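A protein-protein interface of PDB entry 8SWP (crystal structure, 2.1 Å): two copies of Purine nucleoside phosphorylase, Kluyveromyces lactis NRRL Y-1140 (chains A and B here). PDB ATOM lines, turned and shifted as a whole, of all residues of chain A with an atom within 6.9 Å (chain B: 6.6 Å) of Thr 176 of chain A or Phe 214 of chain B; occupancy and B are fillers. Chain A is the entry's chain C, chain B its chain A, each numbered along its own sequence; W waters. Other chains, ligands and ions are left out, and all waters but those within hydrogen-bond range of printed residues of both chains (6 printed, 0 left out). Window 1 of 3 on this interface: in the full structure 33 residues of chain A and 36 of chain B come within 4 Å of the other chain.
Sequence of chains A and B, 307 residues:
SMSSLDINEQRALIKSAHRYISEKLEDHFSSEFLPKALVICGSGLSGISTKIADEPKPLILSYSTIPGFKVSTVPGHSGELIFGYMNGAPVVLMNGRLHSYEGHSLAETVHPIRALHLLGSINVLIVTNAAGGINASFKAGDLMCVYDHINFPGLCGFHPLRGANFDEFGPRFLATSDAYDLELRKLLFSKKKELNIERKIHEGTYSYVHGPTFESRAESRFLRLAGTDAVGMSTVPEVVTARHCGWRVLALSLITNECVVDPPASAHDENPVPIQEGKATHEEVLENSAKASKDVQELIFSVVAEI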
ATOM      1  N   TYR A 147     -20.241  26.929  11.626  1.00  0.00           N
ATOM      2  CA  TYR A 147     -20.057  25.529  11.270  1.00  0.00           C
ATOM      3  C   TYR A 147     -20.886  25.113  10.062  1.00  0.00           C
ATOM      4  O   TYR A 147     -20.873  23.932   9.695  1.00  0.00           O
ATOM      5  CB  TYR A 147     -20.352  24.618  12.477  1.00  0.00           C
ATOM      6  CG  TYR A 147     -21.807  24.405  12.881  1.00  0.00           C
ATOM      7  CD1 TYR A 147     -22.823  25.262  12.466  1.00  0.00           C
ATOM      8  CD2 TYR A 147     -22.154  23.338  13.701  1.00  0.00           C
ATOM      9  CE1 TYR A 147     -24.139  25.048  12.846  1.00  0.00           C
ATOM     10  CE2 TYR A 147     -23.463  23.120  14.088  1.00  0.00           C
ATOM     11  CZ  TYR A 147     -24.451  23.978  13.659  1.00  0.00           C
ATOM     12  OH  TYR A 147     -25.755  23.761  14.043  1.00  0.00           O
ATOM     13  N   ASP A 148     -21.595  26.048   9.436  1.00  0.00           N
ATOM     14  CA  ASP A 148     -22.375  25.807   8.229  1.00  0.00           C
ATOM     15  C   ASP A 148     -22.764  27.160   7.657  1.00  0.00           C
ATOM     16  O   ASP A 148     -22.746  28.174   8.362  1.00  0.00           O
ATOM     17  CB  ASP A 148     -23.619  24.959   8.513  1.00  0.00           C
ATOM     18  CG  ASP A 148     -24.048  24.136   7.316  1.00  0.00           C
ATOM     19  OD1 ASP A 148     -23.423  24.269   6.243  1.00  0.00           O
ATOM     20  OD2 ASP A 148     -25.010  23.352   7.451  1.00  0.00           O
ATOM     21  N   HIS A 149     -23.113  27.173   6.372  1.00  0.00           N
ATOM     22  CA  HIS A 149     -23.531  28.407   5.726  1.00  0.00           C
ATOM     23  C   HIS A 149     -24.620  28.121   4.702  1.00  0.00           C
ATOM     24  O   HIS A 149     -24.860  26.974   4.311  1.00  0.00           O
ATOM     25  CB  HIS A 149     -22.346  29.142   5.074  1.00  0.00           C
ATOM     26  CG  HIS A 149     -21.724  28.419   3.917  1.00  0.00           C
ATOM     27  ND1 HIS A 149     -20.368  28.187   3.833  1.00  0.00           N
ATOM     28  CD2 HIS A 149     -22.262  27.907   2.783  1.00  0.00           C
ATOM     29  CE1 HIS A 149     -20.100  27.547   2.709  1.00  0.00           C
ATOM     30  NE2 HIS A 149     -21.233  27.364   2.054  1.00  0.00           N
ATOM     31  N   HIS A 159     -21.687  33.161  -7.992  1.00  0.00           N
ATOM     32  CA  HIS A 159     -20.872  32.125  -7.310  1.00  0.00           C
ATOM     33  C   HIS A 159     -19.387  32.303  -7.633  1.00  0.00           C
ATOM     34  O   HIS A 159     -19.023  32.486  -8.797  1.00  0.00           O
ATOM     35  CB  HIS A 159     -21.360  30.746  -7.764  1.00  0.00           C
ATOM     36  CG  HIS A 159     -20.945  29.593  -6.926  1.00  0.00           C
ATOM     37  ND1 HIS A 159     -19.645  29.148  -6.855  1.00  0.00           N
ATOM     38  CD2 HIS A 159     -21.660  28.785  -6.144  1.00  0.00           C
ATOM     39  CE1 HIS A 159     -19.590  28.115  -6.035  1.00  0.00           C
ATOM     40  NE2 HIS A 159     -20.803  27.876  -5.597  1.00  0.00           N
ATOM     41  N   PHE A 173     -16.765  20.234  -9.443  1.00  0.00           N
ATOM     42  CA  PHE A 173     -17.883  20.152  -8.481  1.00  0.00           C
ATOM     43  C   PHE A 173     -17.303  19.975  -7.082  1.00  0.00           C
ATOM     44  O   PHE A 173     -16.635  18.972  -6.839  1.00  0.00           O
ATOM     45  CB  PHE A 173     -18.842  19.035  -8.886  1.00  0.00           C
ATOM     46  CG  PHE A 173     -19.380  19.128 -10.289  1.00  0.00           C
ATOM     47  CD1 PHE A 173     -20.364  20.046 -10.610  1.00  0.00           C
ATOM     48  CD2 PHE A 173     -18.908  18.292 -11.284  1.00  0.00           C
ATOM     49  CE1 PHE A 173     -20.860  20.127 -11.898  1.00  0.00           C
ATOM     50  CE2 PHE A 173     -19.402  18.377 -12.573  1.00  0.00           C
ATOM     51  CZ  PHE A 173     -20.375  19.295 -12.877  1.00  0.00           C
ATOM     52  N   LEU A 174     -17.562  20.930  -6.197  1.00  0.00           N
ATOM     53  CA  LEU A 174     -16.959  20.885  -4.842  1.00  0.00           C
ATOM     54  C   LEU A 174     -18.047  20.715  -3.788  1.00  0.00           C
ATOM     55  O   LEU A 174     -19.039  21.433  -3.848  1.00  0.00           O
ATOM     56  CB  LEU A 174     -16.178  22.179  -4.603  1.00  0.00           C
ATOM     57  CG  LEU A 174     -15.683  22.414  -3.177  1.00  0.00           C
ATOM     58  CD1 LEU A 174     -14.372  21.686  -2.934  1.00  0.00           C
ATOM     59  CD2 LEU A 174     -15.526  23.901  -2.901  1.00  0.00           C
ATOM     60  N   ALA A 175     -17.833  19.798  -2.855  1.00  0.00           N
ATOM     61  CA  ALA A 175     -18.787  19.599  -1.752  1.00  0.00           C
ATOM     62  C   ALA A 175     -18.590  20.685  -0.696  1.00  0.00           C
ATOM     63  O   ALA A 175     -17.460  21.159  -0.547  1.00  0.00           O
ATOM     64  CB  ALA A 175     -18.596  18.238  -1.166  1.00  0.00           C
ATOM     65  N   THR A 176     -19.655  21.035   0.017  1.00  0.00           N
ATOM     66  CA  THR A 176     -19.589  22.140   1.006  1.00  0.00           C
ATOM     67  C   THR A 176     -20.102  21.642   2.358  1.00  0.00           C
ATOM     68  O   THR A 176     -20.161  22.450   3.287  1.00  0.00           O
ATOM     69  CB  THR A 176     -20.329  23.374   0.474  1.00  0.00           C
ATOM     70  OG1 THR A 176     -21.639  22.984   0.071  1.00  0.00           O
ATOM     71  CG2 THR A 176     -19.609  24.037  -0.679  1.00  0.00           C
ATOM     72  N   SER A 177     -20.430  20.354   2.453  1.00  0.00           N
ATOM     73  CA  SER A 177     -20.919  19.739   3.715  1.00  0.00           C
ATOM     74  C   SER A 177     -19.776  19.545   4.721  1.00  0.00           C
ATOM     75  O   SER A 177     -20.077  19.331   5.903  1.00  0.00           O
ATOM     76  CB  SER A 177     -21.587  18.424   3.416  1.00  0.00           C
ATOM     77  OG  SER A 177     -20.806  17.638   2.533  1.00  0.00           O
ATOM     78  N   ASP A 178     -18.523  19.590   4.263  1.00  0.00           N
ATOM     79  CA  ASP A 178     -17.338  19.440   5.149  1.00  0.00           C
ATOM     80  C   ASP A 178     -16.525  20.739   5.137  1.00  0.00           C
ATOM     81  O   ASP A 178     -15.304  20.663   5.279  1.00  0.00           O
ATOM     82  CB  ASP A 178     -16.491  18.254   4.695  1.00  0.00           C
ATOM     83  CG  ASP A 178     -15.997  18.346   3.260  1.00  0.00           C
ATOM     84  OD1 ASP A 178     -16.575  19.122   2.479  1.00  0.00           O
ATOM     85  OD2 ASP A 178     -15.032  17.638   2.939  1.00  0.00           O
ATOM     86  N   ALA A 179     -17.182  21.887   4.997  1.00  0.00           N
ATOM     87  CA  ALA A 179     -16.441  23.157   4.826  1.00  0.00           C
ATOM     88  C   ALA A 179     -15.817  23.676   6.122  1.00  0.00           C
ATOM     89  O   ALA A 179     -14.756  24.284   6.032  1.00  0.00           O
ATOM     90  CB  ALA A 179     -17.365  24.188   4.239  1.00  0.00           C
ATOM     91  N   TYR A 180     -16.456  23.458   7.261  1.00  0.00           N
ATOM     92  CA  TYR A 180     -15.954  24.069   8.515  1.00  0.00           C
ATOM     93  C   TYR A 180     -15.289  22.999   9.393  1.00  0.00           C
ATOM     94  O   TYR A 180     -16.005  22.300  10.125  1.00  0.00           O
ATOM     95  CB  TYR A 180     -17.082  24.876   9.164  1.00  0.00           C
ATOM     96  CG  TYR A 180     -17.568  26.017   8.309  1.00  0.00           C
ATOM     97  CD1 TYR A 180     -16.899  27.226   8.296  1.00  0.00           C
ATOM     98  CD2 TYR A 180     -18.673  25.878   7.487  1.00  0.00           C
ATOM     99  CE1 TYR A 180     -17.324  28.276   7.503  1.00  0.00           C
ATOM    100  CE2 TYR A 180     -19.116  26.920   6.692  1.00  0.00           C
ATOM    101  CZ  TYR A 180     -18.437  28.124   6.699  1.00  0.00           C
ATOM    102  OH  TYR A 180     -18.858  29.166   5.918  1.00  0.00           O
ATOM    103  N   VAL A 240     -15.557  29.211   0.200  1.00  0.00           N
ATOM    104  CA  VAL A 240     -15.699  28.286  -0.919  1.00  0.00           C
ATOM    105  C   VAL A 240     -14.405  28.206  -1.720  1.00  0.00           C
ATOM    106  O   VAL A 240     -13.970  27.117  -2.116  1.00  0.00           O
ATOM    107  CB  VAL A 240     -16.890  28.703  -1.801  1.00  0.00           C
ATOM    108  CG1 VAL A 240     -16.877  27.940  -3.115  1.00  0.00           C
ATOM    109  CG2 VAL A 240     -18.198  28.475  -1.060  1.00  0.00           C
ATOM    110  N   ARG A 243     -11.867  26.283   0.296  1.00  0.00           N
ATOM    111  CA  ARG A 243     -12.204  24.865   0.241  1.00  0.00           C
ATOM    112  C   ARG A 243     -11.879  24.279  -1.126  1.00  0.00           C
ATOM    113  O   ARG A 243     -11.442  23.126  -1.228  1.00  0.00           O
ATOM    114  CB  ARG A 243     -13.681  24.659   0.577  1.00  0.00           C
ATOM    115  CG  ARG A 243     -14.018  24.851   2.047  1.00  0.00           C
ATOM    116  CD  ARG A 243     -13.198  23.923   2.931  1.00  0.00           C
ATOM    117  NE  ARG A 243     -13.572  22.525   2.758  1.00  0.00           N
ATOM    118  CZ  ARG A 243     -12.712  21.515   2.753  1.00  0.00           C
ATOM    119  NH1 ARG A 243     -11.413  21.713   2.910  1.00  0.00           N
ATOM    120  NH2 ARG A 243     -13.166  20.275   2.587  1.00  0.00           N
ATOM    121  N   GLY B 211     -25.210  25.861  -8.943  1.00  0.00           N
ATOM    122  CA  GLY B 211     -23.971  25.127  -8.846  1.00  0.00           C
ATOM    123  C   GLY B 211     -22.785  26.067  -8.928  1.00  0.00           C
ATOM    124  O   GLY B 211     -22.932  27.288  -8.830  1.00  0.00           O
ATOM    125  N   PRO B 212     -21.577  25.518  -9.130  1.00  0.00           N
ATOM    126  CA  PRO B 212     -21.264  24.098  -9.308  1.00  0.00           C
ATOM    127  C   PRO B 212     -20.951  23.372  -8.001  1.00  0.00           C
ATOM    128  O   PRO B 212     -20.509  22.223  -8.033  1.00  0.00           O
ATOM    129  CB  PRO B 212     -20.031  24.141 -10.207  1.00  0.00           C
ATOM    130  CG  PRO B 212     -19.312  25.369  -9.741  1.00  0.00           C
ATOM    131  CD  PRO B 212     -20.381  26.360  -9.313  1.00  0.00           C
ATOM    132  N   THR B 213     -21.167  24.036  -6.870  1.00  0.00           N
ATOM    133  CA  THR B 213     -20.939  23.403  -5.582  1.00  0.00           C
ATOM    134  C   THR B 213     -22.098  22.487  -5.220  1.00  0.00           C
ATOM    135  O   THR B 213     -23.256  22.750  -5.556  1.00  0.00           O
ATOM    136  CB  THR B 213     -20.757  24.446  -4.476  1.00  0.00           C
ATOM    137  OG1 THR B 213     -21.763  25.461  -4.596  1.00  0.00           O
ATOM    138  CG2 THR B 213     -19.377  25.076  -4.555  1.00  0.00           C
ATOM    139  N   PHE B 214     -21.776  21.393  -4.537  1.00  0.00           N
ATOM    140  CA  PHE B 214     -22.812  20.605  -3.893  1.00  0.00           C
ATOM    141  C   PHE B 214     -23.317  21.348  -2.663  1.00  0.00           C
ATOM    142  O   PHE B 214     -22.596  22.139  -2.048  1.00  0.00           O
ATOM    143  CB  PHE B 214     -22.281  19.223  -3.509  1.00  0.00           C
ATOM    144  CG  PHE B 214     -22.000  18.332  -4.686  1.00  0.00           C
ATOM    145  CD1 PHE B 214     -23.034  17.861  -5.481  1.00  0.00           C
ATOM    146  CD2 PHE B 214     -20.702  17.965  -4.998  1.00  0.00           C
ATOM    147  CE1 PHE B 214     -22.776  17.041  -6.565  1.00  0.00           C
ATOM    148  CE2 PHE B 214     -20.437  17.145  -6.080  1.00  0.00           C
ATOM    149  CZ  PHE B 214     -21.476  16.682  -6.864  1.00  0.00           C
ATOM    150  N   GLU B 215     -24.575  21.096  -2.311  1.00  0.00           N
ATOM    151  CA  GLU B 215     -25.220  21.877  -1.265  1.00  0.00           C
ATOM    152  C   GLU B 215     -24.589  21.597   0.091  1.00  0.00           C
ATOM    153  O   GLU B 215     -24.217  20.461   0.403  1.00  0.00           O
ATOM    154  CB  GLU B 215     -26.718  21.572  -1.198  1.00  0.00           C
ATOM    155  CG  GLU B 215     -27.524  21.958  -2.429  1.00  0.00           C
ATOM    156  CD  GLU B 215     -27.162  21.125  -3.635  1.00  0.00           C
ATOM    157  OE1 GLU B 215     -26.833  19.938  -3.437  1.00  0.00           O
ATOM    158  OE2 GLU B 215     -27.203  21.650  -4.768  1.00  0.00           O
ATOM    159  N   SER B 216     -24.463  22.646   0.897  1.00  0.00           N
ATOM    160  CA  SER B 216     -24.132  22.464   2.297  1.00  0.00           C
ATOM    161  C   SER B 216     -25.322  21.848   3.028  1.00  0.00           C
ATOM    162  O   SER B 216     -26.433  21.751   2.495  1.00  0.00           O
ATOM    163  CB  SER B 216     -23.737  23.797   2.933  1.00  0.00           C
ATOM    164  OG  SER B 216     -24.850  24.672   3.018  1.00  0.00           O
ATOM    165  N   ARG B 217     -25.081  21.418   4.267  1.00  0.00           N
ATOM    166  CA  ARG B 217     -26.158  20.833   5.059  1.00  0.00           C
ATOM    167  C   ARG B 217     -27.281  21.838   5.288  1.00  0.00           C
ATOM    168  O   ARG B 217     -28.464  21.485   5.217  1.00  0.00           O
ATOM    169  CB  ARG B 217     -25.612  20.321   6.391  1.00  0.00           C
ATOM    170  CG  ARG B 217     -24.509  19.287   6.249  1.00  0.00           C
ATOM    171  CD  ARG B 217     -23.600  19.285   7.464  1.00  0.00           C
ATOM    172  NE  ARG B 217     -22.443  18.418   7.281  1.00  0.00           N
ATOM    173  CZ  ARG B 217     -22.372  17.163   7.705  1.00  0.00           C
ATOM    174  NH1 ARG B 217     -23.378  16.594   8.350  1.00  0.00           N
ATOM    175  NH2 ARG B 217     -21.264  16.464   7.478  1.00  0.00           N
ATOM    176  N   GLU B 219     -27.960  24.400   3.313  1.00  0.00           N
ATOM    177  CA  GLU B 219     -28.620  24.619   2.030  1.00  0.00           C
ATOM    178  C   GLU B 219     -29.575  23.476   1.702  1.00  0.00           C
ATOM    179  O   GLU B 219     -30.691  23.711   1.225  1.00  0.00           O
ATOM    180  CB  GLU B 219     -27.580  24.796   0.924  1.00  0.00           C
ATOM    181  CG  GLU B 219     -26.928  26.174   0.912  1.00  0.00           C
ATOM    182  CD  GLU B 219     -25.572  26.185   0.231  1.00  0.00           C
ATOM    183  OE1 GLU B 219     -25.197  25.162  -0.378  1.00  0.00           O
ATOM    184  OE2 GLU B 219     -24.879  27.222   0.309  1.00  0.00           O
ATOM    185  N   SER B 220     -29.156  22.234   1.961  1.00  0.00           N
ATOM    186  CA  SER B 220     -30.044  21.095   1.742  1.00  0.00           C
ATOM    187  C   SER B 220     -31.229  21.128   2.698  1.00  0.00           C
ATOM    188  O   SER B 220     -32.354  20.785   2.313  1.00  0.00           O
ATOM    189  CB  SER B 220     -29.267  19.787   1.894  1.00  0.00           C
ATOM    190  OG  SER B 220     -28.415  19.566   0.785  1.00  0.00           O
ATOM    191  N   MET B 233     -28.815  20.713 -11.111  1.00  0.00           N
ATOM    192  CA  MET B 233     -28.074  21.865 -11.605  1.00  0.00           C
ATOM    193  C   MET B 233     -28.454  22.271 -13.030  1.00  0.00           C
ATOM    194  O   MET B 233     -27.737  23.045 -13.664  1.00  0.00           O
ATOM    195  CB  MET B 233     -26.575  21.562 -11.541  1.00  0.00           C
ATOM    196  CG  MET B 233     -25.886  21.975 -10.252  1.00  0.00           C
ATOM    197  SD  MET B 233     -23.984  21.524 -10.288  1.00  0.00           S
ATOM    198  CE  MET B 233     -23.772  20.920  -8.440  1.00  0.00           C
ATOM    199  N   ASN B 257     -27.347  10.471  -5.565  1.00  0.00           N
ATOM    200  CA  ASN B 257     -26.760  10.545  -4.234  1.00  0.00           C
ATOM    201  C   ASN B 257     -27.813  11.065  -3.267  1.00  0.00           C
ATOM    202  O   ASN B 257     -28.791  11.702  -3.671  1.00  0.00           O
ATOM    203  CB  ASN B 257     -25.523  11.450  -4.210  1.00  0.00           C
ATOM    204  CG  ASN B 257     -25.823  12.852  -4.696  1.00  0.00           C
ATOM    205  OD1 ASN B 257     -26.151  13.053  -5.864  1.00  0.00           O
ATOM    206  ND2 ASN B 257     -25.722  13.828  -3.802  1.00  0.00           N
ATOM    207  N   LYS B 279     -20.089  12.694   2.017  1.00  0.00           N
ATOM    208  CA  LYS B 279     -20.037  13.876   1.170  1.00  0.00           C
ATOM    209  C   LYS B 279     -20.258  13.508  -0.293  1.00  0.00           C
ATOM    210  O   LYS B 279     -19.893  12.423  -0.752  1.00  0.00           O
ATOM    211  CB  LYS B 279     -18.696  14.595   1.334  1.00  0.00           C
ATOM    212  CG  LYS B 279     -17.510  13.860   0.730  1.00  0.00           C
ATOM    213  CD  LYS B 279     -16.198  14.526   1.107  1.00  0.00           C
ATOM    214  CE  LYS B 279     -16.043  15.866   0.408  1.00  0.00           C
ATOM    215  NZ  LYS B 279     -15.892  15.712  -1.067  1.00  0.00           N
ATOM    216  N   ALA B 280     -20.876  14.431  -1.026  1.00  0.00           N
ATOM    217  CA  ALA B 280     -21.151  14.205  -2.435  1.00  0.00           C
ATOM    218  C   ALA B 280     -19.869  14.298  -3.254  1.00  0.00           C
ATOM    219  O   ALA B 280     -18.948  15.053  -2.931  1.00  0.00           O
ATOM    220  CB  ALA B 280     -22.176  15.214  -2.950  1.00  0.00           C
ATOM    221  N   THR B 281     -19.802  13.509  -4.322  1.00  0.00           N
ATOM    222  CA  THR B 281     -18.659  13.569  -5.216  1.00  0.00           C
ATOM    223  C   THR B 281     -19.127  13.353  -6.646  1.00  0.00           C
ATOM    224  O   THR B 281     -20.147  12.704  -6.896  1.00  0.00           O
ATOM    225  CB  THR B 281     -17.569  12.551  -4.826  1.00  0.00           C
ATOM    226  OG1 THR B 281     -16.298  12.996  -5.319  1.00  0.00           O
ATOM    227  CG2 THR B 281     -17.868  11.176  -5.388  1.00  0.00           C
ATOM    228  N   HIS B 282     -18.377  13.932  -7.580  1.00  0.00           N
ATOM    229  CA  HIS B 282     -18.739  13.855  -8.992  1.00  0.00           C
ATOM    230  C   HIS B 282     -18.651  12.428  -9.515  1.00  0.00           C
ATOM    231  O   HIS B 282     -19.449  12.034 -10.374  1.00  0.00           O
ATOM    232  CB  HIS B 282     -17.844  14.775  -9.821  1.00  0.00           C
ATOM    233  CG  HIS B 282     -18.148  14.754 -11.286  1.00  0.00           C
ATOM    234  ND1 HIS B 282     -19.402  15.028 -11.790  1.00  0.00           N
ATOM    235  CD2 HIS B 282     -17.365  14.480 -12.357  1.00  0.00           C
ATOM    236  CE1 HIS B 282     -19.375  14.931 -13.108  1.00  0.00           C
ATOM    237  NE2 HIS B 282     -18.152  14.599 -13.477  1.00  0.00           N
ATOM    238  N   VAL B 285     -21.758  10.616  -8.742  1.00  0.00           N
ATOM    239  CA  VAL B 285     -22.820  11.052  -9.643  1.00  0.00           C
ATOM    240  C   VAL B 285     -22.675  10.375 -11.000  1.00  0.00           C
ATOM    241  O   VAL B 285     -23.646   9.855 -11.562  1.00  0.00           O
ATOM    242  CB  VAL B 285     -22.814  12.585  -9.775  1.00  0.00           C
ATOM    243  CG1 VAL B 285     -23.782  13.031 -10.859  1.00  0.00           C
ATOM    244  CG2 VAL B 285     -23.157  13.233  -8.442  1.00  0.00           C
HETATM  245  O   HOH W   1     -16.702  16.149  -6.894  1.00  0.00           O
HETATM  246  O   HOH W   2     -20.290  15.528   4.600  1.00  0.00           O
HETATM  247  O   HOH W   3     -21.940  16.594   0.333  1.00  0.00           O
HETATM  248  O   HOH W   4     -22.145  26.345  -0.414  1.00  0.00           O
HETATM  249  O   HOH W   5     -21.741  19.314  -0.209  1.00  0.00           O
HETATM  250  O   HOH W   6     -21.604  27.708  -2.475  1.00  0.00           O
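Of the printed residues of chain B, His 159 of chain A touches Gly 211, Pro 212 and Thr 213.
Of the printed residues of chain B, Ala 175 of chain A touches Phe 214, Lys 279 and Ala 280.
Printed residues of chain B within 4 Å of Thr 176 of chain A: Thr 213, Phe 214, Glu 215 and Ser 216.
Tyr 180 of chain A touches none of the printed residues of chain B.
Printed residues of chain A within 4 Å of Arg 217 of chain B: Asp 148 and Ser 177.
Printed residues of chain A within 4 Å of Met 233 of chain B: Phe 173.
Val 285 of chain B touches none of the printed residues of chain A.
The nearest residue of chain A that does not touch Phe 214 of chain B is Ser 177 of chain A (5.3 Å).
The nearest printed residue of chain B that does not touch Phe 173 of chain A is Thr 213 of chain B (5.2 Å).
No position is printed for both chains.
OG1 of Thr 213 of chain B sits at hydrogen-bond distance from NE2 of His 159 of chain A (2.8 Å).
The backbone NH of Phe 214 of chain B sits at hydrogen-bond distance from the backbone carbonyl oxygen of Leu 174 of chain A, 2.8 Å away.
The side-chain hydroxyl of Thr 176 of chain A is in hydrogen-bond range of the backbone carbonyl oxygen of Phe 214 of chain B (2.5 Å).
The side-chain hydroxyl (OG) of Ser 216 of chain B lies within hydrogen-bond range of the backbone carbonyl oxygen (O) of His 149 of chain A (2.6 Å).
The side-chain hydroxyl of Thr 176 of chain A is in hydrogen-bond range of the backbone NH of Ser 216 of chain B (3.0 Å).
NE of Arg 217 of chain B is in hydrogen-bond range of O of Ser 177 of chain A (2.9 Å).
OD2 of Asp 148 of chain A touches CB of Arg 217 of chain B, 3.3 Å away.
CD2 of His 149 of chain A touches OE2 of Glu 219 of chain B, at 3.7 Å.
His 159 of chain A touches Gly 211 of chain B (CD2 to O, 3.3 Å).
Pro 212 of chain B touches His 159 of chain A.
Phe 173 of chain A touches Pro 212 of chain B.
Phe 214 of chain B touches Phe 173 of chain A (CE2 to CB, 3.7 Å).
Phe 173 of chain A touches Met 233 of chain B.
Ala 175 of chain A touches Ala 280 of chain B.
CG2 of Thr 176 of chain A touches CB of Thr 213 of chain B, at 3.99 Å.
Lys 279 of chain B touches Asp 178 of chain A (CE to OD2, 3.3 Å).
Of the 14 printed residues of chain A, 9 touch a printed residue of chain B.
Hydrophobic or aromatic side chains of chain A within 4 Å of the printed part of chain B: His 149, His 159, Phe 173 and Ala 175.
Hydrophobic or aromatic side chains of chain B within 4 Å of the printed part of chain A: Pro 212, Phe 214, Met 233 and His 282.
Among the printed residues, 24 pairs touch across the chains.
Among the printed residues, no Asp or Glu carboxylate lies within 4 Å of a Lys or Arg side-chain nitrogen of the other chain.
The backbone NH of Ser 216 of chain B sits at hydrogen-bond distance from the side-chain carboxylate of Glu 219 of chain B (2.9 Å).
O of Ser 216 of chain B is in hydrogen-bond range of OG of Ser 220 of chain B, at 3.4 Å.
The side-chain hydroxyl (OH) of Tyr 180 of chain A is in hydrogen-bond range of a ring nitrogen (ND1) of His 149 of chain A (2.8 Å).
NH2 of Arg 243 of chain A lies within salt-bridge range of OD2 of Asp 178 of chain A.
Water W3 lies within hydrogen-bond range of the side-chain hydroxyl of Ser 177 of chain A (2.7 Å) and the backbone NH of Ala 280 of chain B (2.8 Å).
Water W5 lies within hydrogen-bond range of N of Thr 176 of chain A (2.7 Å), O of Glu 215 of chain B (2.8 Å), N of Ser 177 of chain A (3.1 Å) and O of Phe 214 of chain B (3.5 Å).
Water W4 lies within hydrogen-bond range of NE2 of His 149 of chain A (2.8 Å), OE2 of Glu 219 of chain B (3.0 Å) and OG1 of Thr 176 of chain A (3.4 Å).
Water W1 bridges O of Phe 173 of chain A (2.8 Å) and N of His 282 of chain B (2.9 Å).
Water W2 lies within hydrogen-bond range of OG of Ser 177 of chain A (3.0 Å) and NH2 of Arg 217 of chain B (3.2 Å).
Water W6 bridges OG1 of Thr 213 of chain B (3.1 Å) and NE2 of His 159 of chain A (3.2 Å).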
